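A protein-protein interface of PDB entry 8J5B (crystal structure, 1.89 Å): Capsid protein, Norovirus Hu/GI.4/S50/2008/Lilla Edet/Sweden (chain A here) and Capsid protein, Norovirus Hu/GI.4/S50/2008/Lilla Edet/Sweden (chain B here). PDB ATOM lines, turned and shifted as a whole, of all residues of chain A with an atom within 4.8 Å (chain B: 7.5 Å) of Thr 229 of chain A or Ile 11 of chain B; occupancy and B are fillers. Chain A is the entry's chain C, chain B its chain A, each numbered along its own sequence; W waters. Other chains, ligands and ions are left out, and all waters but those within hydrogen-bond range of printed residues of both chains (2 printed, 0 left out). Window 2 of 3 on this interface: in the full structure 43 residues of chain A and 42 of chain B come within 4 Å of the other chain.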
ATOM      1  N   VAL A  55      11.850   9.842 -18.543  1.00  0.00           N
ATOM      2  CA  VAL A  55      11.621   8.431 -18.137  1.00  0.00           C
ATOM      3  C   VAL A  55      10.149   8.094 -18.380  1.00  0.00           C
ATOM      4  O   VAL A  55       9.928   7.069 -19.029  1.00  0.00           O
ATOM      5  CB  VAL A  55      12.054   8.199 -16.676  1.00  0.00           C
ATOM      6  CG1 VAL A  55      11.660   6.817 -16.163  1.00  0.00           C
ATOM      7  CG2 VAL A  55      13.539   8.449 -16.522  1.00  0.00           C
ATOM      8  N   GLN A 225       7.013   4.718 -25.494  1.00  0.00           N
ATOM      9  CA  GLN A 225       7.673   5.209 -24.248  1.00  0.00           C
ATOM     10  C   GLN A 225       7.980   4.023 -23.329  1.00  0.00           C
ATOM     11  O   GLN A 225       9.029   4.040 -22.630  1.00  0.00           O
ATOM     12  CB  GLN A 225       6.824   6.266 -23.522  1.00  0.00           C
ATOM     13  CG  GLN A 225       7.512   6.905 -22.326  1.00  0.00           C
ATOM     14  CD  GLN A 225       8.744   7.689 -22.707  1.00  0.00           C
ATOM     15  OE1 GLN A 225       8.828   8.207 -23.811  1.00  0.00           O
ATOM     16  NE2 GLN A 225       9.681   7.810 -21.771  1.00  0.00           N
ATOM     17  N   GLU A 226       7.086   3.045 -23.231  1.00  0.00           N
ATOM     18  CA  GLU A 226       7.273   1.957 -22.239  1.00  0.00           C
ATOM     19  C   GLU A 226       8.526   1.134 -22.588  1.00  0.00           C
ATOM     20  O   GLU A 226       9.230   0.701 -21.673  1.00  0.00           O
ATOM     21  CB  GLU A 226       5.989   1.137 -22.106  1.00  0.00           C
ATOM     22  CG  GLU A 226       4.863   1.941 -21.460  1.00  0.00           C
ATOM     23  CD  GLU A 226       3.958   2.760 -22.362  1.00  0.00           C
ATOM     24  OE1 GLU A 226       4.099   2.719 -23.632  1.00  0.00           O
ATOM     25  OE2 GLU A 226       3.144   3.495 -21.787  1.00  0.00           O
ATOM     26  N   TYR A 227       8.884   1.011 -23.852  1.00  0.00           N
ATOM     27  CA  TYR A 227      10.177   0.391 -24.272  1.00  0.00           C
ATOM     28  C   TYR A 227      11.340   1.121 -23.622  1.00  0.00           C
ATOM     29  O   TYR A 227      12.201   0.418 -23.026  1.00  0.00           O
ATOM     30  CB  TYR A 227      10.334   0.407 -25.790  1.00  0.00           C
ATOM     31  CG  TYR A 227       9.535  -0.656 -26.485  1.00  0.00           C
ATOM     32  CD1 TYR A 227       8.353  -1.122 -25.930  1.00  0.00           C
ATOM     33  CD2 TYR A 227       9.956  -1.191 -27.700  1.00  0.00           C
ATOM     34  CE1 TYR A 227       7.593  -2.079 -26.566  1.00  0.00           C
ATOM     35  CE2 TYR A 227       9.202  -2.152 -28.352  1.00  0.00           C
ATOM     36  CZ  TYR A 227       8.018  -2.591 -27.782  1.00  0.00           C
ATOM     37  OH  TYR A 227       7.264  -3.536 -28.405  1.00  0.00           O
ATOM     38  N   ILE A 228      11.304   2.475 -23.672  1.00  0.00           N
ATOM     39  CA  ILE A 228      12.410   3.365 -23.215  1.00  0.00           C
ATOM     40  C   ILE A 228      12.568   3.168 -21.704  1.00  0.00           C
ATOM     41  O   ILE A 228      13.691   2.891 -21.256  1.00  0.00           O
ATOM     42  CB  ILE A 228      12.118   4.830 -23.597  1.00  0.00           C
ATOM     43  CG1 ILE A 228      12.166   5.025 -25.115  1.00  0.00           C
ATOM     44  CG2 ILE A 228      13.032   5.802 -22.856  1.00  0.00           C
ATOM     45  CD1 ILE A 228      11.848   6.433 -25.559  1.00  0.00           C
ATOM     46  N   THR A 229      11.454   3.220 -20.957  1.00  0.00           N
ATOM     47  CA  THR A 229      11.466   3.049 -19.476  1.00  0.00           C
ATOM     48  C   THR A 229      12.052   1.689 -19.112  1.00  0.00           C
ATOM     49  O   THR A 229      12.888   1.621 -18.171  1.00  0.00           O
ATOM     50  CB  THR A 229      10.079   3.245 -18.855  1.00  0.00           C
ATOM     51  OG1 THR A 229       9.461   4.369 -19.468  1.00  0.00           O
ATOM     52  CG2 THR A 229      10.168   3.508 -17.368  1.00  0.00           C
ATOM     53  N   HIS A 230      11.628   0.643 -19.811  1.00  0.00           N
ATOM     54  CA  HIS A 230      12.229  -0.717 -19.704  1.00  0.00           C
ATOM     55  C   HIS A 230      13.745  -0.620 -19.864  1.00  0.00           C
ATOM     56  O   HIS A 230      14.497  -1.076 -18.963  1.00  0.00           O
ATOM     57  CB  HIS A 230      11.613  -1.682 -20.726  1.00  0.00           C
ATOM     58  CG  HIS A 230      11.993  -3.111 -20.492  1.00  0.00           C
ATOM     59  ND1 HIS A 230      11.581  -3.816 -19.362  1.00  0.00           N
ATOM     60  CD2 HIS A 230      12.747  -3.970 -21.218  1.00  0.00           C
ATOM     61  CE1 HIS A 230      12.047  -5.054 -19.425  1.00  0.00           C
ATOM     62  NE2 HIS A 230      12.775  -5.174 -20.549  1.00  0.00           N
ATOM     63  N   PHE A 231      14.196  -0.035 -20.952  1.00  0.00           N
ATOM     64  CA  PHE A 231      15.656  -0.006 -21.253  1.00  0.00           C
ATOM     65  C   PHE A 231      16.393   0.723 -20.130  1.00  0.00           C
ATOM     66  O   PHE A 231      17.503   0.232 -19.736  1.00  0.00           O
ATOM     67  CB  PHE A 231      15.968   0.575 -22.626  1.00  0.00           C
ATOM     68  CG  PHE A 231      15.284  -0.091 -23.789  1.00  0.00           C
ATOM     69  CD1 PHE A 231      14.980  -1.447 -23.777  1.00  0.00           C
ATOM     70  CD2 PHE A 231      14.972   0.646 -24.915  1.00  0.00           C
ATOM     71  CE1 PHE A 231      14.315  -2.026 -24.849  1.00  0.00           C
ATOM     72  CE2 PHE A 231      14.336   0.062 -26.000  1.00  0.00           C
ATOM     73  CZ  PHE A 231      14.003  -1.274 -25.966  1.00  0.00           C
ATOM     74  N   ILE A 232      15.796   1.810 -19.597  1.00  0.00           N
ATOM     75  CA  ILE A 232      16.422   2.636 -18.537  1.00  0.00           C
ATOM     76  C   ILE A 232      16.610   1.801 -17.272  1.00  0.00           C
ATOM     77  O   ILE A 232      17.710   1.831 -16.718  1.00  0.00           O
ATOM     78  CB  ILE A 232      15.610   3.921 -18.301  1.00  0.00           C
ATOM     79  CG1 ILE A 232      15.670   4.842 -19.533  1.00  0.00           C
ATOM     80  CG2 ILE A 232      16.087   4.595 -17.026  1.00  0.00           C
ATOM     81  CD1 ILE A 232      15.021   6.184 -19.339  1.00  0.00           C
ATOM     82  N   SER A 233      15.564   1.123 -16.808  1.00  0.00           N
ATOM     83  CA  SER A 233      15.621   0.187 -15.661  1.00  0.00           C
ATOM     84  C   SER A 233      16.603  -0.965 -15.953  1.00  0.00           C
ATOM     85  O   SER A 233      17.449  -1.246 -15.105  1.00  0.00           O
ATOM     86  CB  SER A 233      14.238  -0.338 -15.377  1.00  0.00           C
ATOM     87  OG  SER A 233      14.254  -1.236 -14.283  1.00  0.00           O
ATOM     88  N   VAL B   8      11.233  -5.113  -9.332  1.00  0.00           N
ATOM     89  CA  VAL B   8      10.566  -3.789  -9.414  1.00  0.00           C
ATOM     90  C   VAL B   8      11.484  -2.868 -10.222  1.00  0.00           C
ATOM     91  O   VAL B   8      12.699  -2.899 -10.049  1.00  0.00           O
ATOM     92  CB  VAL B   8      10.274  -3.251  -8.000  1.00  0.00           C
ATOM     93  CG1 VAL B   8       9.610  -1.896  -8.094  1.00  0.00           C
ATOM     94  CG2 VAL B   8       9.395  -4.202  -7.188  1.00  0.00           C
ATOM     95  N   PRO B   9      10.975  -2.041 -11.168  1.00  0.00           N
ATOM     96  CA  PRO B   9      11.866  -1.204 -11.970  1.00  0.00           C
ATOM     97  C   PRO B   9      12.931  -0.492 -11.126  1.00  0.00           C
ATOM     98  O   PRO B   9      12.612  -0.014 -10.070  1.00  0.00           O
ATOM     99  CB  PRO B   9      10.917  -0.210 -12.616  1.00  0.00           C
ATOM    100  CG  PRO B   9       9.650  -1.040 -12.787  1.00  0.00           C
ATOM    101  CD  PRO B   9       9.558  -1.834 -11.497  1.00  0.00           C
ATOM    102  N   ASN B  10      14.149  -0.417 -11.661  1.00  0.00           N
ATOM    103  CA  ASN B  10      15.353   0.214 -11.061  1.00  0.00           C
ATOM    104  C   ASN B  10      15.369   1.699 -11.420  1.00  0.00           C
ATOM    105  O   ASN B  10      16.316   2.141 -12.098  1.00  0.00           O
ATOM    106  CB  ASN B  10      16.635  -0.450 -11.567  1.00  0.00           C
ATOM    107  CG  ASN B  10      17.837  -0.003 -10.775  1.00  0.00           C
ATOM    108  OD1 ASN B  10      17.707   0.341  -9.600  1.00  0.00           O
ATOM    109  ND2 ASN B  10      18.990   0.039 -11.426  1.00  0.00           N
ATOM    110  N   ILE B  11      14.315   2.408 -11.030  1.00  0.00           N
ATOM    111  CA  ILE B  11      14.121   3.845 -11.328  1.00  0.00           C
ATOM    112  C   ILE B  11      13.671   4.560 -10.059  1.00  0.00           C
ATOM    113  O   ILE B  11      12.773   4.093  -9.345  1.00  0.00           O
ATOM    114  CB  ILE B  11      13.109   4.046 -12.464  1.00  0.00           C
ATOM    115  CG1 ILE B  11      13.444   3.183 -13.683  1.00  0.00           C
ATOM    116  CG2 ILE B  11      13.028   5.531 -12.783  1.00  0.00           C
ATOM    117  CD1 ILE B  11      12.411   3.283 -14.802  1.00  0.00           C
ATOM    118  N   PRO B  12      14.274   5.724  -9.750  1.00  0.00           N
ATOM    119  CA  PRO B  12      13.797   6.548  -8.636  1.00  0.00           C
ATOM    120  C   PRO B  12      12.328   6.967  -8.784  1.00  0.00           C
ATOM    121  O   PRO B  12      11.850   7.321  -9.892  1.00  0.00           O
ATOM    122  CB  PRO B  12      14.798   7.719  -8.624  1.00  0.00           C
ATOM    123  CG  PRO B  12      16.065   7.089  -9.234  1.00  0.00           C
ATOM    124  CD  PRO B  12      15.500   6.261 -10.363  1.00  0.00           C
ATOM    125  N   LEU B  13      11.633   6.922  -7.647  1.00  0.00           N
ATOM    126  CA  LEU B  13      10.183   7.215  -7.503  1.00  0.00           C
ATOM    127  C   LEU B  13       9.803   8.525  -8.222  1.00  0.00           C
ATOM    128  O   LEU B  13       8.745   8.564  -8.879  1.00  0.00           O
ATOM    129  CB  LEU B  13       9.928   7.286  -5.999  1.00  0.00           C
ATOM    130  CG  LEU B  13       8.479   7.228  -5.529  1.00  0.00           C
ATOM    131  CD1 LEU B  13       7.681   6.169  -6.264  1.00  0.00           C
ATOM    132  CD2 LEU B  13       8.469   6.966  -4.040  1.00  0.00           C
ATOM    133  N   LYS B  14      10.628   9.568  -8.076  1.00  0.00           N
ATOM    134  CA  LYS B  14      10.368  10.935  -8.587  1.00  0.00           C
ATOM    135  C   LYS B  14      10.197  10.973 -10.116  1.00  0.00           C
ATOM    136  O   LYS B  14       9.678  11.962 -10.576  1.00  0.00           O
ATOM    137  CB  LYS B  14      11.513  11.859  -8.189  1.00  0.00           C
ATOM    138  CG  LYS B  14      12.906  11.311  -8.464  1.00  0.00           C
ATOM    139  CD  LYS B  14      13.867  12.320  -9.007  1.00  0.00           C
ATOM    140  CE  LYS B  14      13.957  13.576  -8.184  1.00  0.00           C
ATOM    141  NZ  LYS B  14      15.137  14.367  -8.596  1.00  0.00           N
ATOM    142  N   TYR B  15      10.648   9.968 -10.888  1.00  0.00           N
ATOM    143  CA  TYR B  15      10.509   9.961 -12.370  1.00  0.00           C
ATOM    144  C   TYR B  15       9.248   9.205 -12.799  1.00  0.00           C
ATOM    145  O   TYR B  15       9.002   9.060 -14.009  1.00  0.00           O
ATOM    146  CB  TYR B  15      11.732   9.314 -13.031  1.00  0.00           C
ATOM    147  CG  TYR B  15      13.013  10.036 -12.745  1.00  0.00           C
ATOM    148  CD1 TYR B  15      13.357  11.184 -13.445  1.00  0.00           C
ATOM    149  CD2 TYR B  15      13.853   9.587 -11.740  1.00  0.00           C
ATOM    150  CE1 TYR B  15      14.530  11.866 -13.175  1.00  0.00           C
ATOM    151  CE2 TYR B  15      15.023  10.259 -11.449  1.00  0.00           C
ATOM    152  CZ  TYR B  15      15.351  11.404 -12.158  1.00  0.00           C
ATOM    153  OH  TYR B  15      16.507  12.041 -11.834  1.00  0.00           O
ATOM    154  N   LEU B  16       8.460   8.732 -11.837  1.00  0.00           N
ATOM    155  CA  LEU B  16       7.371   7.777 -12.124  1.00  0.00           C
ATOM    156  C   LEU B  16       6.033   8.503 -12.026  1.00  0.00           C
ATOM    157  O   LEU B  16       5.980   9.645 -11.472  1.00  0.00           O
ATOM    158  CB  LEU B  16       7.472   6.592 -11.158  1.00  0.00           C
ATOM    159  CG  LEU B  16       8.334   5.405 -11.618  1.00  0.00           C
ATOM    160  CD1 LEU B  16       9.570   5.826 -12.396  1.00  0.00           C
ATOM    161  CD2 LEU B  16       8.741   4.543 -10.430  1.00  0.00           C
ATOM    162  N   GLU B 228       4.319   2.786 -13.785  1.00  0.00           N
ATOM    163  CA  GLU B 228       5.469   2.025 -14.350  1.00  0.00           C
ATOM    164  C   GLU B 228       5.633   0.687 -13.610  1.00  0.00           C
ATOM    165  O   GLU B 228       6.117  -0.272 -14.255  1.00  0.00           O
ATOM    166  CB  GLU B 228       6.741   2.869 -14.324  1.00  0.00           C
ATOM    167  CG  GLU B 228       6.738   3.981 -15.350  1.00  0.00           C
ATOM    168  CD  GLU B 228       5.944   5.235 -15.007  1.00  0.00           C
ATOM    169  OE1 GLU B 228       5.422   5.316 -13.853  1.00  0.00           O
ATOM    170  OE2 GLU B 228       5.831   6.133 -15.893  1.00  0.00           O
ATOM    171  N   TYR B 229       5.259   0.590 -12.325  1.00  0.00           N
ATOM    172  CA  TYR B 229       5.354  -0.684 -11.559  1.00  0.00           C
ATOM    173  C   TYR B 229       4.333  -1.669 -12.146  1.00  0.00           C
ATOM    174  O   TYR B 229       4.663  -2.849 -12.450  1.00  0.00           O
ATOM    175  CB  TYR B 229       5.141  -0.456 -10.062  1.00  0.00           C
ATOM    176  CG  TYR B 229       6.321   0.080  -9.301  1.00  0.00           C
ATOM    177  CD1 TYR B 229       7.358   0.758  -9.919  1.00  0.00           C
ATOM    178  CD2 TYR B 229       6.360  -0.054  -7.933  1.00  0.00           C
ATOM    179  CE1 TYR B 229       8.426   1.245  -9.195  1.00  0.00           C
ATOM    180  CE2 TYR B 229       7.420   0.424  -7.186  1.00  0.00           C
ATOM    181  CZ  TYR B 229       8.448   1.092  -7.821  1.00  0.00           C
ATOM    182  OH  TYR B 229       9.475   1.572  -7.073  1.00  0.00           O
ATOM    183  N   THR B 231       2.943  -1.607 -15.144  1.00  0.00           N
ATOM    184  CA  THR B 231       3.259  -1.945 -16.550  1.00  0.00           C
ATOM    185  C   THR B 231       4.330  -3.046 -16.548  1.00  0.00           C
ATOM    186  O   THR B 231       4.269  -3.944 -17.361  1.00  0.00           O
ATOM    187  CB  THR B 231       3.718  -0.692 -17.316  1.00  0.00           C
ATOM    188  OG1 THR B 231       2.674   0.278 -17.331  1.00  0.00           O
ATOM    189  CG2 THR B 231       4.125  -1.019 -18.739  1.00  0.00           C
ATOM    190  N   TYR B 249      13.353   0.413   0.460  1.00  0.00           N
ATOM    191  CA  TYR B 249      13.461   1.736  -0.178  1.00  0.00           C
ATOM    192  C   TYR B 249      14.923   2.147  -0.057  1.00  0.00           C
ATOM    193  O   TYR B 249      15.409   2.368   1.084  1.00  0.00           O
ATOM    194  CB  TYR B 249      12.513   2.739   0.477  1.00  0.00           C
ATOM    195  CG  TYR B 249      12.345   3.974  -0.361  1.00  0.00           C
ATOM    196  CD1 TYR B 249      11.769   3.883  -1.622  1.00  0.00           C
ATOM    197  CD2 TYR B 249      12.795   5.209   0.068  1.00  0.00           C
ATOM    198  CE1 TYR B 249      11.610   4.995  -2.422  1.00  0.00           C
ATOM    199  CE2 TYR B 249      12.589   6.347  -0.699  1.00  0.00           C
ATOM    200  CZ  TYR B 249      11.995   6.234  -1.949  1.00  0.00           C
ATOM    201  OH  TYR B 249      11.845   7.326  -2.744  1.00  0.00           O
ATOM    202  N   PRO B 252      20.041   5.032  -3.994  1.00  0.00           N
ATOM    203  CA  PRO B 252      20.944   4.427  -4.970  1.00  0.00           C
ATOM    204  C   PRO B 252      22.380   4.986  -4.965  1.00  0.00           C
ATOM    205  O   PRO B 252      23.257   4.330  -5.453  1.00  0.00           O
ATOM    206  CB  PRO B 252      20.302   4.712  -6.349  1.00  0.00           C
ATOM    207  CG  PRO B 252      19.225   5.744  -6.109  1.00  0.00           C
ATOM    208  CD  PRO B 252      18.942   5.766  -4.627  1.00  0.00           C
ATOM    209  N   LEU B 285      12.105  11.420  -2.288  1.00  0.00           N
ATOM    210  CA  LEU B 285      11.419  10.841  -3.476  1.00  0.00           C
ATOM    211  C   LEU B 285      12.443  10.348  -4.510  1.00  0.00           C
ATOM    212  O   LEU B 285      12.050  10.118  -5.648  1.00  0.00           O
ATOM    213  CB  LEU B 285      10.486  11.879  -4.095  1.00  0.00           C
ATOM    214  CG  LEU B 285       9.094  11.977  -3.472  1.00  0.00           C
ATOM    215  CD1 LEU B 285       8.127  11.056  -4.182  1.00  0.00           C
ATOM    216  CD2 LEU B 285       9.115  11.687  -1.975  1.00  0.00           C
ATOM    217  N   ASP B 286      13.714  10.234  -4.158  1.00  0.00           N
ATOM    218  CA  ASP B 286      14.748   9.833  -5.146  1.00  0.00           C
ATOM    219  C   ASP B 286      15.330   8.468  -4.750  1.00  0.00           C
ATOM    220  O   ASP B 286      16.407   8.088  -5.261  1.00  0.00           O
ATOM    221  CB  ASP B 286      15.789  10.936  -5.316  1.00  0.00           C
ATOM    222  CG  ASP B 286      16.486  11.325  -4.029  1.00  0.00           C
ATOM    223  OD1 ASP B 286      16.129  10.745  -2.943  1.00  0.00           O
ATOM    224  OD2 ASP B 286      17.354  12.233  -4.122  1.00  0.00           O
ATOM    225  N   GLY B 287      14.580   7.715  -3.944  1.00  0.00           N
ATOM    226  CA  GLY B 287      14.882   6.315  -3.618  1.00  0.00           C
ATOM    227  C   GLY B 287      14.378   5.396  -4.698  1.00  0.00           C
ATOM    228  O   GLY B 287      13.586   5.854  -5.565  1.00  0.00           O
ATOM    229  N   VAL B 288      14.829   4.143  -4.629  1.00  0.00           N
ATOM    230  CA  VAL B 288      14.396   3.027  -5.509  1.00  0.00           C
ATOM    231  C   VAL B 288      13.825   1.901  -4.635  1.00  0.00           C
ATOM    232  O   VAL B 288      14.492   1.494  -3.637  1.00  0.00           O
ATOM    233  CB  VAL B 288      15.591   2.559  -6.350  1.00  0.00           C
ATOM    234  CG1 VAL B 288      15.205   1.416  -7.256  1.00  0.00           C
ATOM    235  CG2 VAL B 288      16.181   3.713  -7.153  1.00  0.00           C
ATOM    236  N   PHE B 289      12.665   1.371  -5.008  1.00  0.00           N
ATOM    237  CA  PHE B 289      12.094   0.168  -4.344  1.00  0.00           C
ATOM    238  C   PHE B 289      12.791  -1.074  -4.909  1.00  0.00           C
ATOM    239  O   PHE B 289      12.847  -1.222  -6.127  1.00  0.00           O
ATOM    240  CB  PHE B 289      10.575   0.104  -4.490  1.00  0.00           C
ATOM    241  CG  PHE B 289       9.846   0.936  -3.475  1.00  0.00           C
ATOM    242  CD1 PHE B 289       9.940   0.645  -2.122  1.00  0.00           C
ATOM    243  CD2 PHE B 289       9.075   2.019  -3.863  1.00  0.00           C
ATOM    244  CE1 PHE B 289       9.277   1.424  -1.186  1.00  0.00           C
ATOM    245  CE2 PHE B 289       8.402   2.781  -2.929  1.00  0.00           C
ATOM    246  CZ  PHE B 289       8.502   2.478  -1.595  1.00  0.00           C
HETATM  247  O   HOH W   1      19.938  -0.380 -14.593  1.00  0.00           O
HETATM  248  O   HOH W   2       9.936  10.824 -15.917  1.00  0.00           O
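The backbone NH (N) of Asn 10 of chain B sits at hydrogen-bond distance from the side-chain hydroxyl (OG) of Ser 233 of chain A (2.7 Å).
The backbone carbonyl oxygen (O) of Val 55 of chain A is in hydrogen-bond range of the side-chain hydroxyl (OG1) of Thr 229 of chain A, 2.8 Å away. The backbone carbonyl oxygen (O) of Val 55 of chain A lies within hydrogen-bond range of the side-chain amide nitrogen (NE2) of Gln 225 of chain A (2.9 Å). The side-chain hydroxyl of Thr 229 of chain A is in hydrogen-bond range of the backbone carbonyl oxygen of Gln 225 of chain A (3.2 Å).
Among the printed residues, pairs that only touch across the chains: Ser 233 of chain A with Pro 9 of chain B (3.3 Å), Thr 229 of chain A with Ile 11 of chain B (3.4 Å), Val 55 of chain A with Tyr 15 of chain B (3.8 Å), Val 55 of chain A with Ile 11 of chain B (3.9 Å) and Ser 233 of chain A with Ile 11 of chain B (3.99 Å).
Printed residues of chain B within 4 Å of Val 55 of chain A: Ile 11 (3.9 Å) and Tyr 15 (3.8 Å). Printed residues of chain B within 4 Å of Ser 233 of chain A: Pro 9 (3.3 Å), Asn 10 (2.7 Å) and Ile 11 (3.99 Å). Printed residues of chain A within 4 Å of Asn 10 of chain B: Ser 233 (2.7 Å). Leu 13 of chain B touches none of the printed residues of chain A. Printed residues of chain A within 4 Å of Tyr 15 of chain B: Val 55 (3.8 Å). Gly 287 of chain B touches none of the printed residues of chain A. The nearest printed residue of chain A that does not touch Ile 11 of chain B is Ile 232 of chain A (4.5 Å).
Hydrophobic or aromatic side chains of chain A within 4 Å of the printed part of chain B: Val 55. Printed residues of chain B that touch a printed residue of chain A: Pro 9, Asn 10, Ile 11 and Tyr 15.
Water W1 lies within hydrogen-bond range of O of Ser 233 of chain A and ND2 of Asn 10 of chain B. Water W2 lies within hydrogen-bond range of O of Tyr 15 of chain B (2.8 Å) and N of Val 55 of chain A (3.4 Å).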
